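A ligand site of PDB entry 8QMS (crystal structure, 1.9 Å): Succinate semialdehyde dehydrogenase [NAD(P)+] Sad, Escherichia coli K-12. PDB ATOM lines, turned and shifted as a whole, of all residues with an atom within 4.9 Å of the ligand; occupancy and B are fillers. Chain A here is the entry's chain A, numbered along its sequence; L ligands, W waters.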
ATOM      1  N   ILE A 133     -26.495 -20.091   7.247  1.00  0.00           N
ATOM      2  CA  ILE A 133     -26.491 -19.429   8.549  1.00  0.00           C
ATOM      3  C   ILE A 133     -25.071 -18.928   8.796  1.00  0.00           C
ATOM      4  O   ILE A 133     -24.140 -19.732   8.896  1.00  0.00           O
ATOM      5  CB  ILE A 133     -26.952 -20.387   9.652  1.00  0.00           C
ATOM      6  CG1 ILE A 133     -28.192 -21.195   9.214  1.00  0.00           C
ATOM      7  CG2 ILE A 133     -27.229 -19.641  10.937  1.00  0.00           C
ATOM      8  CD1 ILE A 133     -29.459 -20.387   9.114  1.00  0.00           C
ATOM      9  N   MET A 134     -24.902 -17.603   8.919  1.00  0.00           N
ATOM     10  CA  MET A 134     -23.601 -16.978   8.805  1.00  0.00           C
ATOM     11  C   MET A 134     -23.269 -16.075   9.987  1.00  0.00           C
ATOM     12  O   MET A 134     -24.176 -15.579  10.676  1.00  0.00           O
ATOM     13  CB  MET A 134     -23.507 -16.162   7.506  1.00  0.00           C
ATOM     14  CG  MET A 134     -23.503 -17.055   6.256  1.00  0.00           C
ATOM     15  SD  MET A 134     -22.051 -18.127   6.230  1.00  0.00           S
ATOM     16  CE  MET A 134     -22.799 -19.744   5.910  1.00  0.00           C
ATOM     17  N   PRO A 135     -21.959 -15.840  10.248  1.00  0.00           N
ATOM     18  CA  PRO A 135     -21.547 -15.033  11.398  1.00  0.00           C
ATOM     19  C   PRO A 135     -21.103 -13.624  11.016  1.00  0.00           C
ATOM     20  O   PRO A 135     -21.015 -13.301   9.828  1.00  0.00           O
ATOM     21  CB  PRO A 135     -20.354 -15.825  11.933  1.00  0.00           C
ATOM     22  CG  PRO A 135     -19.670 -16.249  10.664  1.00  0.00           C
ATOM     23  CD  PRO A 135     -20.810 -16.535   9.648  1.00  0.00           C
ATOM     24  N   TRP A 136     -20.755 -12.804  12.024  1.00  0.00           N
ATOM     25  CA  TRP A 136     -20.452 -11.385  11.828  1.00  0.00           C
ATOM     26  C   TRP A 136     -18.982 -11.080  11.584  1.00  0.00           C
ATOM     27  O   TRP A 136     -18.659  -9.937  11.233  1.00  0.00           O
ATOM     28  CB  TRP A 136     -20.914 -10.571  13.055  1.00  0.00           C
ATOM     29  CG  TRP A 136     -20.450 -11.163  14.357  1.00  0.00           C
ATOM     30  CD1 TRP A 136     -21.177 -11.937  15.216  1.00  0.00           C
ATOM     31  CD2 TRP A 136     -19.130 -11.069  14.925  1.00  0.00           C
ATOM     32  NE1 TRP A 136     -20.405 -12.320  16.288  1.00  0.00           N
ATOM     33  CE2 TRP A 136     -19.140 -11.797  16.131  1.00  0.00           C
ATOM     34  CE3 TRP A 136     -17.944 -10.433  14.534  1.00  0.00           C
ATOM     35  CZ2 TRP A 136     -18.016 -11.920  16.947  1.00  0.00           C
ATOM     36  CZ3 TRP A 136     -16.809 -10.562  15.344  1.00  0.00           C
ATOM     37  CH2 TRP A 136     -16.861 -11.290  16.537  1.00  0.00           C
ATOM     38  N   ASN A 137     -18.065 -12.040  11.765  1.00  0.00           N
ATOM     39  CA  ASN A 137     -16.645 -11.660  11.779  1.00  0.00           C
ATOM     40  C   ASN A 137     -16.116 -11.336  10.386  1.00  0.00           C
ATOM     41  O   ASN A 137     -15.256 -10.463  10.245  1.00  0.00           O
ATOM     42  CB  ASN A 137     -15.811 -12.746  12.469  1.00  0.00           C
ATOM     43  CG  ASN A 137     -15.761 -14.046  11.709  1.00  0.00           C
ATOM     44  OD1 ASN A 137     -16.715 -14.439  11.025  1.00  0.00           O
ATOM     45  ND2 ASN A 137     -14.633 -14.758  11.829  1.00  0.00           N
ATOM     46  N   GLN A 142     -17.763 -14.508   4.418  1.00  0.00           N
ATOM     47  CA  GLN A 142     -18.412 -15.763   4.798  1.00  0.00           C
ATOM     48  C   GLN A 142     -19.607 -16.052   3.889  1.00  0.00           C
ATOM     49  O   GLN A 142     -19.841 -17.203   3.487  1.00  0.00           O
ATOM     50  CB  GLN A 142     -18.860 -15.745   6.261  1.00  0.00           C
ATOM     51  CG  GLN A 142     -17.747 -15.574   7.285  1.00  0.00           C
ATOM     52  CD  GLN A 142     -16.619 -16.573   7.133  1.00  0.00           C
ATOM     53  OE1 GLN A 142     -16.813 -17.689   6.665  1.00  0.00           O
ATOM     54  NE2 GLN A 142     -15.416 -16.166   7.533  1.00  0.00           N
ATOM     55  N   ARG A 145     -18.132 -16.953   0.314  1.00  0.00           N
ATOM     56  CA  ARG A 145     -17.378 -18.202   0.289  1.00  0.00           C
ATOM     57  C   ARG A 145     -18.256 -19.378  -0.123  1.00  0.00           C
ATOM     58  O   ARG A 145     -17.800 -20.298  -0.817  1.00  0.00           O
ATOM     59  CB  ARG A 145     -16.751 -18.464   1.660  1.00  0.00           C
ATOM     60  CG  ARG A 145     -15.846 -19.690   1.715  1.00  0.00           C
ATOM     61  CD  ARG A 145     -15.218 -19.876   3.106  1.00  0.00           C
ATOM     62  NE  ARG A 145     -16.116 -20.565   4.024  1.00  0.00           N
ATOM     63  CZ  ARG A 145     -15.873 -20.745   5.315  1.00  0.00           C
ATOM     64  NH1 ARG A 145     -14.774 -20.291   5.882  1.00  0.00           N
ATOM     65  NH2 ARG A 145     -16.775 -21.397   6.060  1.00  0.00           N
ATOM     66  N   LYS A 160     -29.419 -16.410   6.096  1.00  0.00           N
ATOM     67  CA  LYS A 160     -29.816 -15.944   7.410  1.00  0.00           C
ATOM     68  C   LYS A 160     -28.547 -15.413   8.084  1.00  0.00           C
ATOM     69  O   LYS A 160     -27.758 -16.196   8.638  1.00  0.00           O
ATOM     70  CB  LYS A 160     -30.477 -17.042   8.242  1.00  0.00           C
ATOM     71  CG  LYS A 160     -31.558 -16.551   9.212  1.00  0.00           C
ATOM     72  CD  LYS A 160     -31.005 -15.607  10.272  1.00  0.00           C
ATOM     73  CE  LYS A 160     -29.910 -16.286  11.122  1.00  0.00           C
ATOM     74  NZ  LYS A 160     -29.390 -15.379  12.194  1.00  0.00           N
ATOM     75  N   HIS A 161     -28.347 -14.107   8.026  1.00  0.00           N
ATOM     76  CA  HIS A 161     -27.116 -13.502   8.521  1.00  0.00           C
ATOM     77  C   HIS A 161     -27.223 -13.223  10.024  1.00  0.00           C
ATOM     78  O   HIS A 161     -28.291 -13.265  10.624  1.00  0.00           O
ATOM     79  CB  HIS A 161     -26.794 -12.223   7.763  1.00  0.00           C
ATOM     80  CG  HIS A 161     -25.327 -12.012   7.531  1.00  0.00           C
ATOM     81  ND1 HIS A 161     -24.370 -12.575   8.346  1.00  0.00           N
ATOM     82  CD2 HIS A 161     -24.664 -11.329   6.579  1.00  0.00           C
ATOM     83  CE1 HIS A 161     -23.172 -12.234   7.910  1.00  0.00           C
ATOM     84  NE2 HIS A 161     -23.319 -11.476   6.836  1.00  0.00           N
ATOM     85  N   ALA A 162     -26.071 -12.927  10.629  1.00  0.00           N
ATOM     86  CA  ALA A 162     -26.022 -12.632  12.050  1.00  0.00           C
ATOM     87  C   ALA A 162     -26.750 -11.314  12.330  1.00  0.00           C
ATOM     88  O   ALA A 162     -26.705 -10.387  11.514  1.00  0.00           O
ATOM     89  CB  ALA A 162     -24.575 -12.558  12.540  1.00  0.00           C
ATOM     90  N   PRO A 163     -27.446 -11.212  13.468  1.00  0.00           N
ATOM     91  CA  PRO A 163     -28.375 -10.081  13.669  1.00  0.00           C
ATOM     92  C   PRO A 163     -27.694  -8.733  13.900  1.00  0.00           C
ATOM     93  O   PRO A 163     -28.384  -7.707  13.882  1.00  0.00           O
ATOM     94  CB  PRO A 163     -29.206 -10.512  14.885  1.00  0.00           C
ATOM     95  CG  PRO A 163     -28.348 -11.523  15.609  1.00  0.00           C
ATOM     96  CD  PRO A 163     -27.562 -12.220  14.537  1.00  0.00           C
ATOM     97  N   ASN A 193     -34.505 -17.606  15.633  1.00  0.00           N
ATOM     98  CA  ASN A 193     -34.080 -18.998  15.668  1.00  0.00           C
ATOM     99  C   ASN A 193     -35.227 -19.943  15.341  1.00  0.00           C
ATOM    100  O   ASN A 193     -35.026 -20.976  14.695  1.00  0.00           O
ATOM    101  CB  ASN A 193     -33.458 -19.338  17.029  1.00  0.00           C
ATOM    102  CG  ASN A 193     -32.091 -18.698  17.223  1.00  0.00           C
ATOM    103  OD1 ASN A 193     -31.498 -18.146  16.298  1.00  0.00           O
ATOM    104  ND2 ASN A 193     -31.559 -18.785  18.450  1.00  0.00           N
ATOM    105  N   VAL A 196     -35.603 -20.149  11.590  1.00  0.00           N
ATOM    106  CA  VAL A 196     -34.636 -21.098  11.043  1.00  0.00           C
ATOM    107  C   VAL A 196     -35.137 -22.526  11.227  1.00  0.00           C
ATOM    108  O   VAL A 196     -35.055 -23.348  10.297  1.00  0.00           O
ATOM    109  CB  VAL A 196     -33.253 -20.891  11.695  1.00  0.00           C
ATOM    110  CG1 VAL A 196     -32.326 -22.063  11.395  1.00  0.00           C
ATOM    111  CG2 VAL A 196     -32.642 -19.571  11.217  1.00  0.00           C
ATOM    112  N   THR A 211     -21.884 -21.550   9.342  1.00  0.00           N
ATOM    113  CA  THR A 211     -20.583 -21.044   9.752  1.00  0.00           C
ATOM    114  C   THR A 211     -20.819 -20.271  11.052  1.00  0.00           C
ATOM    115  O   THR A 211     -21.507 -19.248  11.059  1.00  0.00           O
ATOM    116  CB  THR A 211     -19.986 -20.158   8.664  1.00  0.00           C
ATOM    117  OG1 THR A 211     -19.691 -20.967   7.525  1.00  0.00           O
ATOM    118  CG2 THR A 211     -18.723 -19.517   9.147  1.00  0.00           C
ATOM    119  N   GLY A 212     -20.302 -20.801  12.157  1.00  0.00           N
ATOM    120  CA  GLY A 212     -20.605 -20.198  13.447  1.00  0.00           C
ATOM    121  C   GLY A 212     -19.955 -20.950  14.575  1.00  0.00           C
ATOM    122  O   GLY A 212     -18.963 -21.655  14.382  1.00  0.00           O
ATOM    123  N   SER A 213     -20.514 -20.780  15.764  1.00  0.00           N
ATOM    124  CA  SER A 213     -19.948 -21.382  16.962  1.00  0.00           C
ATOM    125  C   SER A 213     -20.289 -22.869  17.036  1.00  0.00           C
ATOM    126  O   SER A 213     -21.161 -23.379  16.330  1.00  0.00           O
ATOM    127  CB  SER A 213     -20.441 -20.678  18.219  1.00  0.00           C
ATOM    128  OG  SER A 213     -21.838 -20.861  18.378  1.00  0.00           O
ATOM    129  N   ARG A 215     -21.753 -24.225  19.524  1.00  0.00           N
ATOM    130  CA  ARG A 215     -23.104 -24.328  20.056  1.00  0.00           C
ATOM    131  C   ARG A 215     -24.159 -24.193  18.956  1.00  0.00           C
ATOM    132  O   ARG A 215     -25.146 -24.924  18.931  1.00  0.00           O
ATOM    133  CB  ARG A 215     -23.310 -23.264  21.133  1.00  0.00           C
ATOM    134  CG  ARG A 215     -24.696 -23.248  21.761  1.00  0.00           C
ATOM    135  CD  ARG A 215     -24.888 -21.987  22.620  1.00  0.00           C
ATOM    136  NE  ARG A 215     -24.987 -20.784  21.804  1.00  0.00           N
ATOM    137  CZ  ARG A 215     -23.986 -19.955  21.533  1.00  0.00           C
ATOM    138  NH1 ARG A 215     -22.771 -20.154  22.034  1.00  0.00           N
ATOM    139  NH2 ARG A 215     -24.206 -18.912  20.745  1.00  0.00           N
ATOM    140  N   ALA A 216     -23.954 -23.241  18.038  1.00  0.00           N
ATOM    141  CA  ALA A 216     -24.894 -23.077  16.939  1.00  0.00           C
ATOM    142  C   ALA A 216     -24.881 -24.284  16.013  1.00  0.00           C
ATOM    143  O   ALA A 216     -25.936 -24.749  15.566  1.00  0.00           O
ATOM    144  CB  ALA A 216     -24.573 -21.809  16.156  1.00  0.00           C
ATOM    145  N   ALA A 219     -26.826 -27.108  17.585  1.00  0.00           N
ATOM    146  CA  ALA A 219     -28.258 -26.800  17.573  1.00  0.00           C
ATOM    147  C   ALA A 219     -28.839 -26.988  16.173  1.00  0.00           C
ATOM    148  O   ALA A 219     -29.868 -27.649  16.002  1.00  0.00           O
ATOM    149  CB  ALA A 219     -28.483 -25.370  18.068  1.00  0.00           C
ATOM    150  N   ILE A 220     -28.190 -26.422  15.167  1.00  0.00           N
ATOM    151  CA  ILE A 220     -28.696 -26.478  13.801  1.00  0.00           C
ATOM    152  C   ILE A 220     -28.447 -27.846  13.174  1.00  0.00           C
ATOM    153  O   ILE A 220     -29.309 -28.377  12.462  1.00  0.00           O
ATOM    154  CB  ILE A 220     -28.082 -25.352  12.968  1.00  0.00           C
ATOM    155  CG1 ILE A 220     -28.424 -23.985  13.586  1.00  0.00           C
ATOM    156  CG2 ILE A 220     -28.570 -25.437  11.528  1.00  0.00           C
ATOM    157  CD1 ILE A 220     -27.640 -22.829  12.984  1.00  0.00           C
ATOM    158  N   GLN A 223     -31.046 -30.349  13.983  1.00  0.00           N
ATOM    159  CA  GLN A 223     -32.297 -30.117  13.266  1.00  0.00           C
ATOM    160  C   GLN A 223     -32.195 -30.543  11.816  1.00  0.00           C
ATOM    161  O   GLN A 223     -33.154 -31.082  11.255  1.00  0.00           O
ATOM    162  CB  GLN A 223     -32.683 -28.638  13.367  1.00  0.00           C
ATOM    163  CG  GLN A 223     -32.911 -28.144  14.773  1.00  0.00           C
ATOM    164  CD  GLN A 223     -33.316 -26.678  14.780  1.00  0.00           C
ATOM    165  OE1 GLN A 223     -34.411 -26.330  14.365  1.00  0.00           O
ATOM    166  NE2 GLN A 223     -32.422 -25.819  15.252  1.00  0.00           N
ATOM    167  N   GLU A 234     -19.118 -25.482   9.652  1.00  0.00           N
ATOM    168  CA  GLU A 234     -17.817 -24.827   9.751  1.00  0.00           C
ATOM    169  C   GLU A 234     -17.849 -24.031  11.056  1.00  0.00           C
ATOM    170  O   GLU A 234     -18.322 -22.896  11.097  1.00  0.00           O
ATOM    171  CB  GLU A 234     -17.560 -23.933   8.544  1.00  0.00           C
ATOM    172  CG  GLU A 234     -17.471 -24.699   7.228  1.00  0.00           C
ATOM    173  CD  GLU A 234     -16.030 -25.015   6.860  1.00  0.00           C
ATOM    174  OE1 GLU A 234     -15.117 -24.539   7.563  1.00  0.00           O
ATOM    175  OE2 GLU A 234     -15.818 -25.730   5.856  1.00  0.00           O
ATOM    176  N   LEU A 235     -17.323 -24.636  12.125  1.00  0.00           N
ATOM    177  CA  LEU A 235     -17.552 -24.121  13.450  1.00  0.00           C
ATOM    178  C   LEU A 235     -16.271 -23.465  14.003  1.00  0.00           C
ATOM    179  O   LEU A 235     -15.396 -23.032  13.245  1.00  0.00           O
ATOM    180  CB  LEU A 235     -18.105 -25.235  14.321  1.00  0.00           C
ATOM    181  CG  LEU A 235     -19.290 -25.951  13.656  1.00  0.00           C
ATOM    182  CD1 LEU A 235     -19.822 -27.084  14.502  1.00  0.00           C
ATOM    183  CD2 LEU A 235     -20.406 -24.949  13.314  1.00  0.00           C
ATOM    184  N   GLY A 236     -16.181 -23.393  15.322  1.00  0.00           N
ATOM    185  CA  GLY A 236     -15.081 -22.674  15.937  1.00  0.00           C
ATOM    186  C   GLY A 236     -13.741 -23.370  15.753  1.00  0.00           C
ATOM    187  O   GLY A 236     -13.632 -24.493  15.242  1.00  0.00           O
ATOM    188  N   GLY A 237     -12.693 -22.667  16.161  1.00  0.00           N
ATOM    189  CA  GLY A 237     -11.358 -23.215  16.151  1.00  0.00           C
ATOM    190  C   GLY A 237     -10.577 -22.759  17.357  1.00  0.00           C
ATOM    191  O   GLY A 237     -10.888 -21.754  17.993  1.00  0.00           O
ATOM    192  N   VAL A 267     -11.093 -14.495  14.402  1.00  0.00           N
ATOM    193  CA  VAL A 267     -10.886 -15.352  13.229  1.00  0.00           C
ATOM    194  C   VAL A 267     -11.025 -16.804  13.647  1.00  0.00           C
ATOM    195  O   VAL A 267     -10.454 -17.233  14.654  1.00  0.00           O
ATOM    196  CB  VAL A 267      -9.507 -15.095  12.577  1.00  0.00           C
ATOM    197  CG1 VAL A 267      -9.324 -16.021  11.383  1.00  0.00           C
ATOM    198  CG2 VAL A 267      -9.374 -13.649  12.155  1.00  0.00           C
ATOM    199  N   CYS A 268     -11.790 -17.570  12.864  1.00  0.00           N
ATOM    200  CA  CYS A 268     -12.004 -18.984  13.160  1.00  0.00           C
ATOM    201  C   CYS A 268     -10.700 -19.766  13.144  1.00  0.00           C
ATOM    202  O   CYS A 268     -10.415 -20.537  14.066  1.00  0.00           O
ATOM    203  CB  CYS A 268     -12.975 -19.588  12.154  1.00  0.00           C
ATOM    204  SG  CYS A 268     -12.495 -19.236  10.455  1.00  0.00           S
ATOM    205  N   ARG A 312     -18.732  -7.142  19.528  1.00  0.00           N
ATOM    206  CA  ARG A 312     -19.911  -7.203  20.387  1.00  0.00           C
ATOM    207  C   ARG A 312     -19.518  -6.949  21.833  1.00  0.00           C
ATOM    208  O   ARG A 312     -18.585  -7.585  22.347  1.00  0.00           O
ATOM    209  CB  ARG A 312     -20.606  -8.555  20.277  1.00  0.00           C
ATOM    210  CG  ARG A 312     -21.142  -8.902  18.900  1.00  0.00           C
ATOM    211  CD  ARG A 312     -22.540  -9.517  18.969  1.00  0.00           C
ATOM    212  NE  ARG A 312     -22.713 -10.450  20.071  1.00  0.00           N
ATOM    213  CZ  ARG A 312     -22.934 -11.754  19.942  1.00  0.00           C
ATOM    214  NH1 ARG A 312     -23.035 -12.319  18.743  1.00  0.00           N
ATOM    215  NH2 ARG A 312     -23.075 -12.502  21.033  1.00  0.00           N
ATOM    216  N   LEU A 315     -19.526 -10.033  24.013  1.00  0.00           N
ATOM    217  CA  LEU A 315     -18.424 -10.967  23.769  1.00  0.00           C
ATOM    218  C   LEU A 315     -17.114 -10.457  24.372  1.00  0.00           C
ATOM    219  O   LEU A 315     -16.253 -11.265  24.744  1.00  0.00           O
ATOM    220  CB  LEU A 315     -18.283 -11.212  22.279  1.00  0.00           C
ATOM    221  CG  LEU A 315     -19.532 -11.871  21.686  1.00  0.00           C
ATOM    222  CD1 LEU A 315     -19.365 -12.174  20.204  1.00  0.00           C
ATOM    223  CD2 LEU A 315     -19.852 -13.139  22.469  1.00  0.00           C
ATOM    224  N   GLU A 365     -12.446 -21.604  22.939  1.00  0.00           N
ATOM    225  CA  GLU A 365     -12.039 -20.693  21.869  1.00  0.00           C
ATOM    226  C   GLU A 365     -11.953 -19.266  22.419  1.00  0.00           C
ATOM    227  O   GLU A 365     -12.931 -18.749  22.964  1.00  0.00           O
ATOM    228  CB  GLU A 365     -13.021 -20.757  20.699  1.00  0.00           C
ATOM    229  CG  GLU A 365     -12.707 -19.750  19.583  1.00  0.00           C
ATOM    230  CD  GLU A 365     -13.627 -19.874  18.374  1.00  0.00           C
ATOM    231  OE1 GLU A 365     -14.834 -20.138  18.579  1.00  0.00           O
ATOM    232  OE2 GLU A 365     -13.151 -19.715  17.226  1.00  0.00           O
ATOM    233  N   PHE A 367     -11.982 -15.871  21.333  1.00  0.00           N
ATOM    234  CA  PHE A 367     -12.368 -15.206  20.085  1.00  0.00           C
ATOM    235  C   PHE A 367     -12.164 -13.694  20.189  1.00  0.00           C
ATOM    236  O   PHE A 367     -13.090 -12.896  20.068  1.00  0.00           O
ATOM    237  CB  PHE A 367     -13.816 -15.549  19.743  1.00  0.00           C
ATOM    238  CG  PHE A 367     -14.106 -15.480  18.272  1.00  0.00           C
ATOM    239  CD1 PHE A 367     -13.486 -16.361  17.399  1.00  0.00           C
ATOM    240  CD2 PHE A 367     -14.980 -14.532  17.766  1.00  0.00           C
ATOM    241  CE1 PHE A 367     -13.757 -16.301  16.033  1.00  0.00           C
ATOM    242  CE2 PHE A 367     -15.250 -14.467  16.412  1.00  0.00           C
ATOM    243  CZ  PHE A 367     -14.624 -15.355  15.542  1.00  0.00           C
ATOM    244  N   LEU A 393      -9.657 -27.226  13.516  1.00  0.00           N
ATOM    245  CA  LEU A 393      -9.860 -26.523  12.252  1.00  0.00           C
ATOM    246  C   LEU A 393      -8.572 -26.493  11.430  1.00  0.00           C
ATOM    247  O   LEU A 393      -8.502 -27.074  10.343  1.00  0.00           O
ATOM    248  CB  LEU A 393     -10.389 -25.102  12.508  1.00  0.00           C
ATOM    249  CG  LEU A 393     -10.822 -24.290  11.281  1.00  0.00           C
ATOM    250  CD1 LEU A 393     -11.812 -25.094  10.432  1.00  0.00           C
ATOM    251  CD2 LEU A 393     -11.438 -22.965  11.721  1.00  0.00           C
ATOM    252  N   PHE A 431     -11.103 -25.981   2.767  1.00  0.00           N
ATOM    253  CA  PHE A 431     -11.204 -25.341   4.064  1.00  0.00           C
ATOM    254  C   PHE A 431     -12.283 -26.044   4.884  1.00  0.00           C
ATOM    255  O   PHE A 431     -13.398 -26.235   4.393  1.00  0.00           O
ATOM    256  CB  PHE A 431     -11.505 -23.841   3.938  1.00  0.00           C
ATOM    257  CG  PHE A 431     -11.449 -23.094   5.244  1.00  0.00           C
ATOM    258  CD1 PHE A 431     -12.553 -23.009   6.068  1.00  0.00           C
ATOM    259  CD2 PHE A 431     -10.267 -22.497   5.651  1.00  0.00           C
ATOM    260  CE1 PHE A 431     -12.487 -22.318   7.282  1.00  0.00           C
ATOM    261  CE2 PHE A 431     -10.196 -21.818   6.855  1.00  0.00           C
ATOM    262  CZ  PHE A 431     -11.306 -21.732   7.664  1.00  0.00           C
HETATM  263  P1  LIG L   1     -22.825 -17.674  16.600  1.00  0.00           P
HETATM  264  O1  LIG L   1     -22.952 -19.122  16.663  1.00  0.00           O
HETATM  265  O2  LIG L   1     -23.244 -17.090  18.017  1.00  0.00           O
HETATM  266  O3  LIG L   1     -23.829 -17.104  15.490  1.00  0.00           O
HETATM  267  C1  LIG L   1     -23.547 -17.711  14.234  1.00  0.00           C
HETATM  268  C2  LIG L   1     -24.796 -17.683  13.346  1.00  0.00           C
HETATM  269  O4  LIG L   1     -25.674 -18.742  13.739  1.00  0.00           O
HETATM  270  C3  LIG L   1     -25.606 -16.381  13.483  1.00  0.00           C
HETATM  271  O5  LIG L   1     -26.251 -16.075  12.257  1.00  0.00           O
HETATM  272  C4  LIG L   1     -26.646 -16.739  14.571  1.00  0.00           C
HETATM  273  O6  LIG L   1     -27.813 -15.938  14.483  1.00  0.00           O
HETATM  274  C5  LIG L   1     -26.948 -18.192  14.134  1.00  0.00           C
HETATM  275  N1  LIG L   1     -27.465 -19.014  15.218  1.00  0.00           N
HETATM  276  C6  LIG L   1     -26.876 -19.240  16.419  1.00  0.00           C
HETATM  277  N2  LIG L   1     -27.610 -20.056  17.118  1.00  0.00           N
HETATM  278  C7  LIG L   1     -28.701 -20.397  16.405  1.00  0.00           C
HETATM  279  C8  LIG L   1     -29.822 -21.209  16.631  1.00  0.00           C
HETATM  280  N3  LIG L   1     -29.980 -21.894  17.812  1.00  0.00           N
HETATM  281  N4  LIG L   1     -30.735 -21.312  15.661  1.00  0.00           N
HETATM  282  C9  LIG L   1     -30.596 -20.667  14.524  1.00  0.00           C
HETATM  283  N5  LIG L   1     -29.575 -19.896  14.270  1.00  0.00           N
HETATM  284  C10 LIG L   1     -28.611 -19.736  15.170  1.00  0.00           C
HETATM  285  O7  LIG L   1     -21.284 -17.357  16.236  1.00  0.00           O
HETATM  286  P2  LIG L   1     -20.862 -15.844  15.886  1.00  0.00           P
HETATM  287  O8  LIG L   1     -20.572 -15.058  17.171  1.00  0.00           O
HETATM  288  O9  LIG L   1     -21.899 -15.081  15.055  1.00  0.00           O
HETATM  289  O10 LIG L   1     -19.514 -15.957  14.993  1.00  0.00           O
HETATM  290  C11 LIG L   1     -18.423 -16.452  15.765  1.00  0.00           C
HETATM  291  C12 LIG L   1     -18.147 -17.946  15.515  1.00  0.00           C
HETATM  292  O11 LIG L   1     -18.062 -18.234  14.104  1.00  0.00           O
HETATM  293  C13 LIG L   1     -16.771 -18.315  16.107  1.00  0.00           C
HETATM  294  O12 LIG L   1     -16.884 -19.489  16.894  1.00  0.00           O
HETATM  295  C14 LIG L   1     -15.916 -18.540  14.842  1.00  0.00           C
HETATM  296  O13 LIG L   1     -14.832 -19.427  15.094  1.00  0.00           O
HETATM  297  C15 LIG L   1     -16.974 -19.145  13.913  1.00  0.00           C
HETATM  298  N6  LIG L   1     -16.515 -19.121  12.531  1.00  0.00           N
HETATM  299  C16 LIG L   1     -16.225 -20.238  11.895  1.00  0.00           C
HETATM  300  C17 LIG L   1     -15.773 -20.198  10.569  1.00  0.00           C
HETATM  301  C18 LIG L   1     -15.427 -21.425   9.815  1.00  0.00           C
HETATM  302  O14 LIG L   1     -15.342 -21.371   8.612  1.00  0.00           O
HETATM  303  N7  LIG L   1     -15.194 -22.589  10.446  1.00  0.00           N
HETATM  304  C19 LIG L   1     -15.648 -18.967   9.934  1.00  0.00           C
HETATM  305  C20 LIG L   1     -15.967 -17.828  10.649  1.00  0.00           C
HETATM  306  C21 LIG L   1     -16.408 -17.951  11.950  1.00  0.00           C
HETATM  307  O   HOH W   1     -24.385 -14.070  15.805  1.00  0.00           O
HETATM  308  O   HOH W   2     -29.326 -16.420  16.421  1.00  0.00           O
HETATM  309  O   HOH W   3     -25.318 -15.340  17.939  1.00  0.00           O
HETATM  310  O   HOH W   4     -16.929 -22.087  18.656  1.00  0.00           O
HETATM  311  O   HOH W   5     -33.007 -23.093  15.439  1.00  0.00           O
HETATM  312  O   HOH W   6     -28.523 -22.265  20.514  1.00  0.00           O
HETATM  313  O   HOH W   7     -16.567 -18.400  19.903  1.00  0.00           O
HETATM  314  O   HOH W   8     -13.012 -16.740  10.369  1.00  0.00           O
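The backbone carbonyl oxygen (O) of Met 134 is in hydrogen-bond range of an oxygen (O5) of the ligand (2.7 Å). An oxygen (O1) of the ligand lies within hydrogen-bond range of the backbone NH (N) of Ser 213 (3.1 Å). The side-chain hydroxyl of Ser 213 sits at hydrogen-bond distance from an oxygen (O1) of the ligand (2.7 Å). The side-chain carboxylate of Glu 365 is in hydrogen-bond range of an oxygen (O13) of the ligand (2.7 Å). The side-chain amino group (NZ) of Lys 160 lies within hydrogen-bond range of an oxygen (O6) of the ligand (2.8 Å). A nitrogen (N7) of the ligand is in hydrogen-bond range of the backbone carbonyl oxygen (O) of Leu 235, 2.8 Å away. The indole nitrogen of Trp 136 is in hydrogen-bond range of an oxygen (O8) of the ligand, at 2.9 Å. An oxygen (O14) of the ligand lies within hydrogen-bond range of the guanidinium group (NH2) of Arg 145 (2.9 Å). The backbone carbonyl oxygen of Glu 234 lies close to a nitrogen (N7) of the ligand, at 3.2 Å. The side-chain carboxylate of Glu 234 lies close to a nitrogen (N7) of the ligand (3.5 Å). The side-chain amide oxygen (OD1) of Asn 193 lies close to a nitrogen (N5) of the ligand (3.3 Å). The guanidinium group (NH2) of Arg 215 lies within salt-bridge range of an oxygen (O2) of the ligand (3.4 Å).
The backbone NH of Met 134 sits at hydrogen-bond distance from the backbone carbonyl oxygen of Lys 160 (3.2 Å). O of Met 134 is in hydrogen-bond range of N of Ala 162, 3.3 Å away. The side-chain carboxylate (OE2) of Glu 365 sits at hydrogen-bond distance from the backbone NH (N) of Gly 237, at 3.2 Å. The side-chain carboxylate (OE1) of Glu 234 lies within salt-bridge range of the guanidinium group (NH2) of Arg 145 (3.9 Å). The guanidinium group of Arg 145 is in hydrogen-bond range of the side-chain hydroxyl of Thr 211 (3.3 Å). The backbone carbonyl oxygen of Glu 234 sits at hydrogen-bond distance from the backbone NH of Gly 212. The backbone carbonyl oxygen (O) of Gly 212 sits at hydrogen-bond distance from the backbone NH (N) of Gly 236 (3.4 Å). O of Ala 219 lies within hydrogen-bond range of NE2 of Gln 223, at 3.2 Å.
Merely in contact with the ligand: Pro 135 (3.2 Å), Ala 216 (3.2 Å), Cys 268 (3.2 Å), Thr 211 (3.2 Å), Gly 212 (3.2 Å), Phe 431 (3.3 Å), Ile 133 (3.3 Å), Phe 367 (3.3 Å), Gly 236 (3.4 Å), Ala 162 (3.5 Å), Asn 137 (3.5 Å), Gln 142 (3.6 Å), Pro 163 (3.7 Å), Ile 220 (3.7 Å), His 161 (3.8 Å), Ala 219 (3.8 Å), Val 196 (3.8 Å) and Leu 393 (3.98 Å). Within 4 Å of the ligand: Ile 133, Met 134, Pro 135, Trp 136, Asn 137, Gln 142, Arg 145, Lys 160, His 161, Ala 162, Pro 163, Asn 193, Val 196, Thr 211, Gly 212, Ser 213, Arg 215, Ala 216, Ala 219, Ile 220, Glu 234, Leu 235, Gly 236, Cys 268, Glu 365, Phe 367, Leu 393 and Phe 431. Along chain A the residues within 4 Å of the ligand span positions 133 to 431.
Water W2 bridges an oxygen (O6) of the ligand and the side-chain amide oxygen of Asn 193. Water W5 lies within hydrogen-bond range of the side-chain amide nitrogen of Gln 223 (2.8 Å), a nitrogen (N4) of the ligand (2.9 Å) and the backbone carbonyl oxygen of Asn 193 (3.0 Å). Water W4 bridges OE1 of Glu 365 (2.9 Å) and O12 of the ligand (3.1 Å). Water W8 bridges the side-chain sulfur (SG) of Cys 268 (2.6 Å) and the side-chain amide nitrogen (ND2) of Asn 137 (2.9 Å). Water W7 lies within hydrogen-bond range of the side-chain carboxylate (OE1) of Glu 365 (2.8 Å) and an oxygen (O12) of the ligand (3.2 Å).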
